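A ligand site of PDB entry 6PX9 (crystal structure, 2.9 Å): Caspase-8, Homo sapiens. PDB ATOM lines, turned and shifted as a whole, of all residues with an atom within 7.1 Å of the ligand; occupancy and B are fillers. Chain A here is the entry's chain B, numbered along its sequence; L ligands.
SG of Cys 144 is bonded to C8 of the ligand (1.8 Å).
The guanidinium group of Arg 44 sits close to an oxygen (O3) of the ligand (3.0 Å).
N of Cys 144 lies within hydrogen-bond range of O of Ser 100, at 3.4 Å.
NH2 of Arg 44 lies within hydrogen-bond range of OG1 of Thr 47 (3.0 Å).
OE1 of Gln 207 sits close to O of Leu 49.
The side-chain carboxylate (OD1) of Asp 50 lies within hydrogen-bond range of the indole nitrogen (NE1) of Trp 204 (2.8 Å).
The side-chain amide oxygen (OE1) of Gln 142 lies close to the side-chain carboxylate (OD2) of Asp 50 (3.0 Å).
OD1 of Asp 50 lies close to OE1 of Gln 207 (3.2 Å).
O of Asp 43 lies within hydrogen-bond range of ND2 of Asn 45, at 3.1 Å.
The backbone NH (N) of Val 190 sits at hydrogen-bond distance from the backbone carbonyl oxygen (O) of Ala 143.
Merely in contact with the ligand: Leu 49 (3.2 Å), Asp 50 (3.3 Å), Gly 46 (3.3 Å), Trp 204 (3.3 Å), Gln 142 (3.3 Å), Asn 45 (3.4 Å), Val 190 (3.5 Å), His 48 (3.8 Å) and Thr 47 (3.9 Å).
Of the 21 residues printed, 11 come within 4 Å of the ligand.
The nearest printed residue that does not touch the ligand is Tyr 205 (4.6 Å).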
ATOM      1  N   ASP A  43     -25.972  -9.905  18.431  1.00  0.00           N
ATOM      2  CA  ASP A  43     -26.378  -8.529  18.423  1.00  0.00           C
ATOM      3  C   ASP A  43     -25.106  -7.747  18.142  1.00  0.00           C
ATOM      4  O   ASP A  43     -24.087  -8.016  18.736  1.00  0.00           O
ATOM      5  CB  ASP A  43     -26.887  -8.132  19.792  1.00  0.00           C
ATOM      6  CG  ASP A  43     -28.288  -8.557  20.033  1.00  0.00           C
ATOM      7  OD1 ASP A  43     -28.932  -9.054  19.112  1.00  0.00           O
ATOM      8  OD2 ASP A  43     -28.753  -8.391  21.158  1.00  0.00           O
ATOM      9  N   ARG A  44     -25.166  -6.702  17.327  1.00  0.00           N
ATOM     10  CA  ARG A  44     -23.956  -5.976  16.989  1.00  0.00           C
ATOM     11  C   ARG A  44     -23.569  -5.004  18.080  1.00  0.00           C
ATOM     12  O   ARG A  44     -23.791  -3.819  17.973  1.00  0.00           O
ATOM     13  CB  ARG A  44     -24.115  -5.252  15.661  1.00  0.00           C
ATOM     14  CG  ARG A  44     -23.791  -6.080  14.431  1.00  0.00           C
ATOM     15  CD  ARG A  44     -23.964  -5.267  13.172  1.00  0.00           C
ATOM     16  NE  ARG A  44     -23.243  -4.023  13.261  1.00  0.00           N
ATOM     17  CZ  ARG A  44     -21.991  -3.855  12.895  1.00  0.00           C
ATOM     18  NH1 ARG A  44     -21.301  -4.870  12.405  1.00  0.00           N
ATOM     19  NH2 ARG A  44     -21.426  -2.684  13.010  1.00  0.00           N
ATOM     20  N   ASN A  45     -22.964  -5.524  19.117  1.00  0.00           N
ATOM     21  CA  ASN A  45     -22.547  -4.733  20.246  1.00  0.00           C
ATOM     22  C   ASN A  45     -21.336  -3.903  19.926  1.00  0.00           C
ATOM     23  O   ASN A  45     -20.341  -4.406  19.456  1.00  0.00           O
ATOM     24  CB  ASN A  45     -22.263  -5.651  21.434  1.00  0.00           C
ATOM     25  CG  ASN A  45     -23.471  -6.444  21.841  1.00  0.00           C
ATOM     26  OD1 ASN A  45     -24.486  -5.874  22.210  1.00  0.00           O
ATOM     27  ND2 ASN A  45     -23.373  -7.752  21.782  1.00  0.00           N
ATOM     28  N   GLY A  46     -21.416  -2.635  20.246  1.00  0.00           N
ATOM     29  CA  GLY A  46     -20.372  -1.682  19.962  1.00  0.00           C
ATOM     30  C   GLY A  46     -20.578  -0.881  18.694  1.00  0.00           C
ATOM     31  O   GLY A  46     -19.889   0.120  18.498  1.00  0.00           O
ATOM     32  N   THR A  47     -21.519  -1.293  17.847  1.00  0.00           N
ATOM     33  CA  THR A  47     -21.834  -0.509  16.658  1.00  0.00           C
ATOM     34  C   THR A  47     -22.252   0.904  17.003  1.00  0.00           C
ATOM     35  O   THR A  47     -22.153   1.796  16.152  1.00  0.00           O
ATOM     36  CB  THR A  47     -22.939  -1.202  15.839  1.00  0.00           C
ATOM     37  OG1 THR A  47     -22.990  -0.628  14.525  1.00  0.00           O
ATOM     38  CG2 THR A  47     -24.285  -1.049  16.517  1.00  0.00           C
ATOM     39  N   HIS A  48     -22.695   1.146  18.242  1.00  0.00           N
ATOM     40  CA  HIS A  48     -23.008   2.485  18.705  1.00  0.00           C
ATOM     41  C   HIS A  48     -21.779   3.357  18.892  1.00  0.00           C
ATOM     42  O   HIS A  48     -21.912   4.498  19.342  1.00  0.00           O
ATOM     43  CB  HIS A  48     -23.790   2.406  20.030  1.00  0.00           C
ATOM     44  CG  HIS A  48     -23.094   1.604  21.084  1.00  0.00           C
ATOM     45  ND1 HIS A  48     -22.177   2.154  21.954  1.00  0.00           N
ATOM     46  CD2 HIS A  48     -23.192   0.288  21.418  1.00  0.00           C
ATOM     47  CE1 HIS A  48     -21.736   1.219  22.768  1.00  0.00           C
ATOM     48  NE2 HIS A  48     -22.335   0.078  22.473  1.00  0.00           N
ATOM     49  N   LEU A  49     -20.586   2.858  18.557  1.00  0.00           N
ATOM     50  CA  LEU A  49     -19.368   3.657  18.543  1.00  0.00           C
ATOM     51  C   LEU A  49     -18.988   4.098  17.140  1.00  0.00           C
ATOM     52  O   LEU A  49     -18.507   5.222  16.951  1.00  0.00           O
ATOM     53  CB  LEU A  49     -18.207   2.875  19.160  1.00  0.00           C
ATOM     54  CG  LEU A  49     -18.287   2.596  20.669  1.00  0.00           C
ATOM     55  CD1 LEU A  49     -18.265   1.105  20.971  1.00  0.00           C
ATOM     56  CD2 LEU A  49     -17.182   3.321  21.432  1.00  0.00           C
ATOM     57  N   ASP A  50     -19.188   3.235  16.133  1.00  0.00           N
ATOM     58  CA  ASP A  50     -19.036   3.660  14.749  1.00  0.00           C
ATOM     59  C   ASP A  50     -20.016   4.780  14.405  1.00  0.00           C
ATOM     60  O   ASP A  50     -19.634   5.777  13.796  1.00  0.00           O
ATOM     61  CB  ASP A  50     -19.253   2.471  13.803  1.00  0.00           C
ATOM     62  CG  ASP A  50     -18.140   1.450  13.874  1.00  0.00           C
ATOM     63  OD1 ASP A  50     -16.965   1.857  13.965  1.00  0.00           O
ATOM     64  OD2 ASP A  50     -18.443   0.234  13.827  1.00  0.00           O
ATOM     65  N   LEU A  99     -24.355   0.232   8.829  1.00  0.00           N
ATOM     66  CA  LEU A  99     -23.633  -0.604   9.742  1.00  0.00           C
ATOM     67  C   LEU A  99     -24.598  -1.702  10.073  1.00  0.00           C
ATOM     68  O   LEU A  99     -25.614  -1.453  10.651  1.00  0.00           O
ATOM     69  CB  LEU A  99     -23.272   0.187  10.973  1.00  0.00           C
ATOM     70  CG  LEU A  99     -22.520   1.465  10.680  1.00  0.00           C
ATOM     71  CD1 LEU A  99     -22.838   2.492  11.724  1.00  0.00           C
ATOM     72  CD2 LEU A  99     -21.044   1.235  10.644  1.00  0.00           C
ATOM     73  N   SER A 100     -24.225  -2.913   9.729  1.00  0.00           N
ATOM     74  CA  SER A 100     -25.014  -4.140   9.886  1.00  0.00           C
ATOM     75  C   SER A 100     -24.172  -5.336   9.510  1.00  0.00           C
ATOM     76  O   SER A 100     -22.971  -5.259   9.498  1.00  0.00           O
ATOM     77  CB  SER A 100     -26.183  -4.106   8.926  1.00  0.00           C
ATOM     78  OG  SER A 100     -27.155  -5.053   9.257  1.00  0.00           O
ATOM     79  N   HIS A 101     -24.794  -6.475   9.290  1.00  0.00           N
ATOM     80  CA  HIS A 101     -24.030  -7.633   8.805  1.00  0.00           C
ATOM     81  C   HIS A 101     -24.755  -8.516   7.816  1.00  0.00           C
ATOM     82  O   HIS A 101     -25.950  -8.595   7.871  1.00  0.00           O
ATOM     83  CB  HIS A 101     -23.362  -8.422   9.929  1.00  0.00           C
ATOM     84  CG  HIS A 101     -24.296  -8.936  10.965  1.00  0.00           C
ATOM     85  ND1 HIS A 101     -23.861  -9.329  12.217  1.00  0.00           N
ATOM     86  CD2 HIS A 101     -25.623  -9.117  10.949  1.00  0.00           C
ATOM     87  CE1 HIS A 101     -24.898  -9.732  12.922  1.00  0.00           C
ATOM     88  NE2 HIS A 101     -25.977  -9.619  12.173  1.00  0.00           N
ATOM     89  N   GLN A 142     -20.279  -1.481   6.237  1.00  0.00           N
ATOM     90  CA  GLN A 142     -19.436  -2.291   7.113  1.00  0.00           C
ATOM     91  C   GLN A 142     -20.299  -3.447   7.627  1.00  0.00           C
ATOM     92  O   GLN A 142     -20.906  -3.351   8.705  1.00  0.00           O
ATOM     93  CB  GLN A 142     -18.865  -1.458   8.258  1.00  0.00           C
ATOM     94  CG  GLN A 142     -17.878  -2.202   9.137  1.00  0.00           C
ATOM     95  CD  GLN A 142     -17.451  -1.396  10.338  1.00  0.00           C
ATOM     96  OE1 GLN A 142     -18.258  -0.712  10.967  1.00  0.00           O
ATOM     97  NE2 GLN A 142     -16.163  -1.453  10.658  1.00  0.00           N
ATOM     98  N   ALA A 143     -20.331  -4.537   6.866  1.00  0.00           N
ATOM     99  CA  ALA A 143     -21.099  -5.724   7.201  1.00  0.00           C
ATOM    100  C   ALA A 143     -20.152  -6.822   7.687  1.00  0.00           C
ATOM    101  O   ALA A 143     -19.184  -7.148   6.998  1.00  0.00           O
ATOM    102  CB  ALA A 143     -21.907  -6.212   6.004  1.00  0.00           C
ATOM    103  N   CYS A 144     -20.447  -7.384   8.858  1.00  0.00           N
ATOM    104  CA  CYS A 144     -19.645  -8.448   9.436  1.00  0.00           C
ATOM    105  C   CYS A 144     -20.049  -9.806   8.861  1.00  0.00           C
ATOM    106  O   CYS A 144     -21.219 -10.059   8.548  1.00  0.00           O
ATOM    107  CB  CYS A 144     -19.798  -8.462  10.959  1.00  0.00           C
ATOM    108  SG  CYS A 144     -20.013  -6.815  11.692  1.00  0.00           S
ATOM    109  N   GLN A 145     -19.071 -10.687   8.736  1.00  0.00           N
ATOM    110  CA  GLN A 145     -19.290 -12.007   8.157  1.00  0.00           C
ATOM    111  C   GLN A 145     -19.639 -13.034   9.232  1.00  0.00           C
ATOM    112  O   GLN A 145     -20.803 -13.400   9.399  1.00  0.00           O
ATOM    113  CB  GLN A 145     -18.069 -12.458   7.370  1.00  0.00           C
ATOM    114  N   ALA A 188     -16.680  -2.941   3.352  1.00  0.00           N
ATOM    115  CA  ALA A 188     -15.741  -3.817   4.047  1.00  0.00           C
ATOM    116  C   ALA A 188     -16.433  -5.121   4.438  1.00  0.00           C
ATOM    117  O   ALA A 188     -17.300  -5.125   5.328  1.00  0.00           O
ATOM    118  CB  ALA A 188     -15.156  -3.125   5.271  1.00  0.00           C
ATOM    119  N   VAL A 190     -16.379  -8.193   6.611  1.00  0.00           N
ATOM    120  CA  VAL A 190     -15.764  -8.285   7.927  1.00  0.00           C
ATOM    121  C   VAL A 190     -16.343  -9.427   8.758  1.00  0.00           C
ATOM    122  O   VAL A 190     -15.612 -10.183   9.402  1.00  0.00           O
ATOM    123  CB  VAL A 190     -15.915  -6.944   8.688  1.00  0.00           C
ATOM    124  CG1 VAL A 190     -15.935  -7.169  10.184  1.00  0.00           C
ATOM    125  CG2 VAL A 190     -14.800  -5.985   8.287  1.00  0.00           C
ATOM    126  N   TRP A 204     -10.306  -0.440  13.288  1.00  0.00           N
ATOM    127  CA  TRP A 204     -11.040  -1.082  12.209  1.00  0.00           C
ATOM    128  C   TRP A 204     -11.478  -0.113  11.138  1.00  0.00           C
ATOM    129  O   TRP A 204     -11.073   1.031  11.140  1.00  0.00           O
ATOM    130  CB  TRP A 204     -12.180  -1.930  12.733  1.00  0.00           C
ATOM    131  CG  TRP A 204     -13.184  -1.226  13.492  1.00  0.00           C
ATOM    132  CD1 TRP A 204     -14.354  -0.786  13.048  1.00  0.00           C
ATOM    133  CD2 TRP A 204     -13.137  -0.914  14.877  1.00  0.00           C
ATOM    134  NE1 TRP A 204     -15.044  -0.179  14.029  1.00  0.00           N
ATOM    135  CE2 TRP A 204     -14.309  -0.251  15.179  1.00  0.00           C
ATOM    136  CE3 TRP A 204     -12.201  -1.121  15.885  1.00  0.00           C
ATOM    137  CZ2 TRP A 204     -14.585   0.206  16.459  1.00  0.00           C
ATOM    138  CZ3 TRP A 204     -12.473  -0.652  17.137  1.00  0.00           C
ATOM    139  CH2 TRP A 204     -13.651  -0.011  17.418  1.00  0.00           C
ATOM    140  N   TYR A 205     -12.319  -0.562  10.234  1.00  0.00           N
ATOM    141  CA  TYR A 205     -12.637   0.261   9.089  1.00  0.00           C
ATOM    142  C   TYR A 205     -13.291   1.567   9.264  1.00  0.00           C
ATOM    143  O   TYR A 205     -12.735   2.542   8.829  1.00  0.00           O
ATOM    144  CB  TYR A 205     -13.470  -0.531   8.105  1.00  0.00           C
ATOM    145  CG  TYR A 205     -13.924   0.263   6.922  1.00  0.00           C
ATOM    146  CD1 TYR A 205     -13.064   1.089   6.281  1.00  0.00           C
ATOM    147  CD2 TYR A 205     -15.203   0.160   6.444  1.00  0.00           C
ATOM    148  CE1 TYR A 205     -13.465   1.811   5.195  1.00  0.00           C
ATOM    149  CE2 TYR A 205     -15.602   0.880   5.372  1.00  0.00           C
ATOM    150  CZ  TYR A 205     -14.719   1.700   4.749  1.00  0.00           C
ATOM    151  OH  TYR A 205     -15.102   2.427   3.675  1.00  0.00           O
ATOM    152  N   ILE A 206     -14.369   1.647  10.016  1.00  0.00           N
ATOM    153  CA  ILE A 206     -15.070   2.903  10.116  1.00  0.00           C
ATOM    154  C   ILE A 206     -14.430   3.874  11.049  1.00  0.00           C
ATOM    155  O   ILE A 206     -14.561   5.063  10.887  1.00  0.00           O
ATOM    156  CB  ILE A 206     -16.508   2.726  10.509  1.00  0.00           C
ATOM    157  CG1 ILE A 206     -17.268   2.032   9.418  1.00  0.00           C
ATOM    158  CG2 ILE A 206     -17.103   4.078  10.705  1.00  0.00           C
ATOM    159  CD1 ILE A 206     -17.818   2.941   8.361  1.00  0.00           C
ATOM    160  N   GLN A 207     -13.766   3.373  12.071  1.00  0.00           N
ATOM    161  CA  GLN A 207     -13.057   4.229  13.004  1.00  0.00           C
ATOM    162  C   GLN A 207     -11.811   4.829  12.369  1.00  0.00           C
ATOM    163  O   GLN A 207     -11.462   5.985  12.644  1.00  0.00           O
ATOM    164  CB  GLN A 207     -12.695   3.442  14.264  1.00  0.00           C
ATOM    165  CG  GLN A 207     -13.896   2.991  15.055  1.00  0.00           C
ATOM    166  CD  GLN A 207     -14.600   4.130  15.752  1.00  0.00           C
ATOM    167  OE1 GLN A 207     -15.745   4.450  15.437  1.00  0.00           O
ATOM    168  NE2 GLN A 207     -13.930   4.741  16.724  1.00  0.00           N
HETATM  169  C1  LIG L   1     -16.713  -1.976  17.694  1.00  0.00           C
HETATM  170  C2  LIG L   1     -17.857  -1.698  16.690  1.00  0.00           C
HETATM  171  C3  LIG L   1     -15.408  -2.053  22.193  1.00  0.00           C
HETATM  172  C4  LIG L   1     -16.127  -4.181  19.073  1.00  0.00           C
HETATM  173  C5  LIG L   1     -16.312  -3.438  20.452  1.00  0.00           C
HETATM  174  C6  LIG L   1     -16.612  -2.140  22.878  1.00  0.00           C
HETATM  175  C7  LIG L   1     -16.182  -4.037  16.456  1.00  0.00           C
HETATM  176  C8  LIG L   1     -18.862  -6.490  13.041  1.00  0.00           C
HETATM  177  C9  LIG L   1     -18.780  -5.562  14.245  1.00  0.00           C
HETATM  178  C10 LIG L   1     -16.283  -4.971  13.738  1.00  0.00           C
HETATM  179  C11 LIG L   1     -15.496  -6.119  13.844  1.00  0.00           C
HETATM  180  C12 LIG L   1     -14.319  -6.232  13.091  1.00  0.00           C
HETATM  181  C13 LIG L   1     -13.919  -5.201  12.231  1.00  0.00           C
HETATM  182  C14 LIG L   1     -14.703  -4.053  12.139  1.00  0.00           C
HETATM  183  C15 LIG L   1     -15.878  -3.935  12.885  1.00  0.00           C
HETATM  184  C16 LIG L   1     -17.540  -3.937  15.776  1.00  0.00           C
HETATM  185  C17 LIG L   1     -17.810  -2.535  15.449  1.00  0.00           C
HETATM  186  C18 LIG L   1     -15.250  -2.699  20.980  1.00  0.00           C
HETATM  187  C19 LIG L   1     -17.666  -2.886  22.349  1.00  0.00           C
HETATM  188  C20 LIG L   1     -17.513  -3.537  21.129  1.00  0.00           C
HETATM  189  C21 LIG L   1     -16.002  -0.232  24.460  1.00  0.00           C
HETATM  190  C22 LIG L   1     -16.823   1.053  24.386  1.00  0.00           C
HETATM  191  C23 LIG L   1     -18.728  -0.087  24.972  1.00  0.00           C
HETATM  192  C24 LIG L   1     -18.038  -1.455  24.897  1.00  0.00           C
HETATM  193  N1  LIG L   1     -16.325  -3.420  17.802  1.00  0.00           N
HETATM  194  N2  LIG L   1     -16.772  -1.446  24.172  1.00  0.00           N
HETATM  195  N3  LIG L   1     -17.555  -4.834  14.556  1.00  0.00           N
HETATM  196  O1  LIG L   1     -15.828  -5.325  19.028  1.00  0.00           O
HETATM  197  O2  LIG L   1     -18.171   0.846  24.135  1.00  0.00           O
HETATM  198  O3  LIG L   1     -19.736  -5.415  14.939  1.00  0.00           O
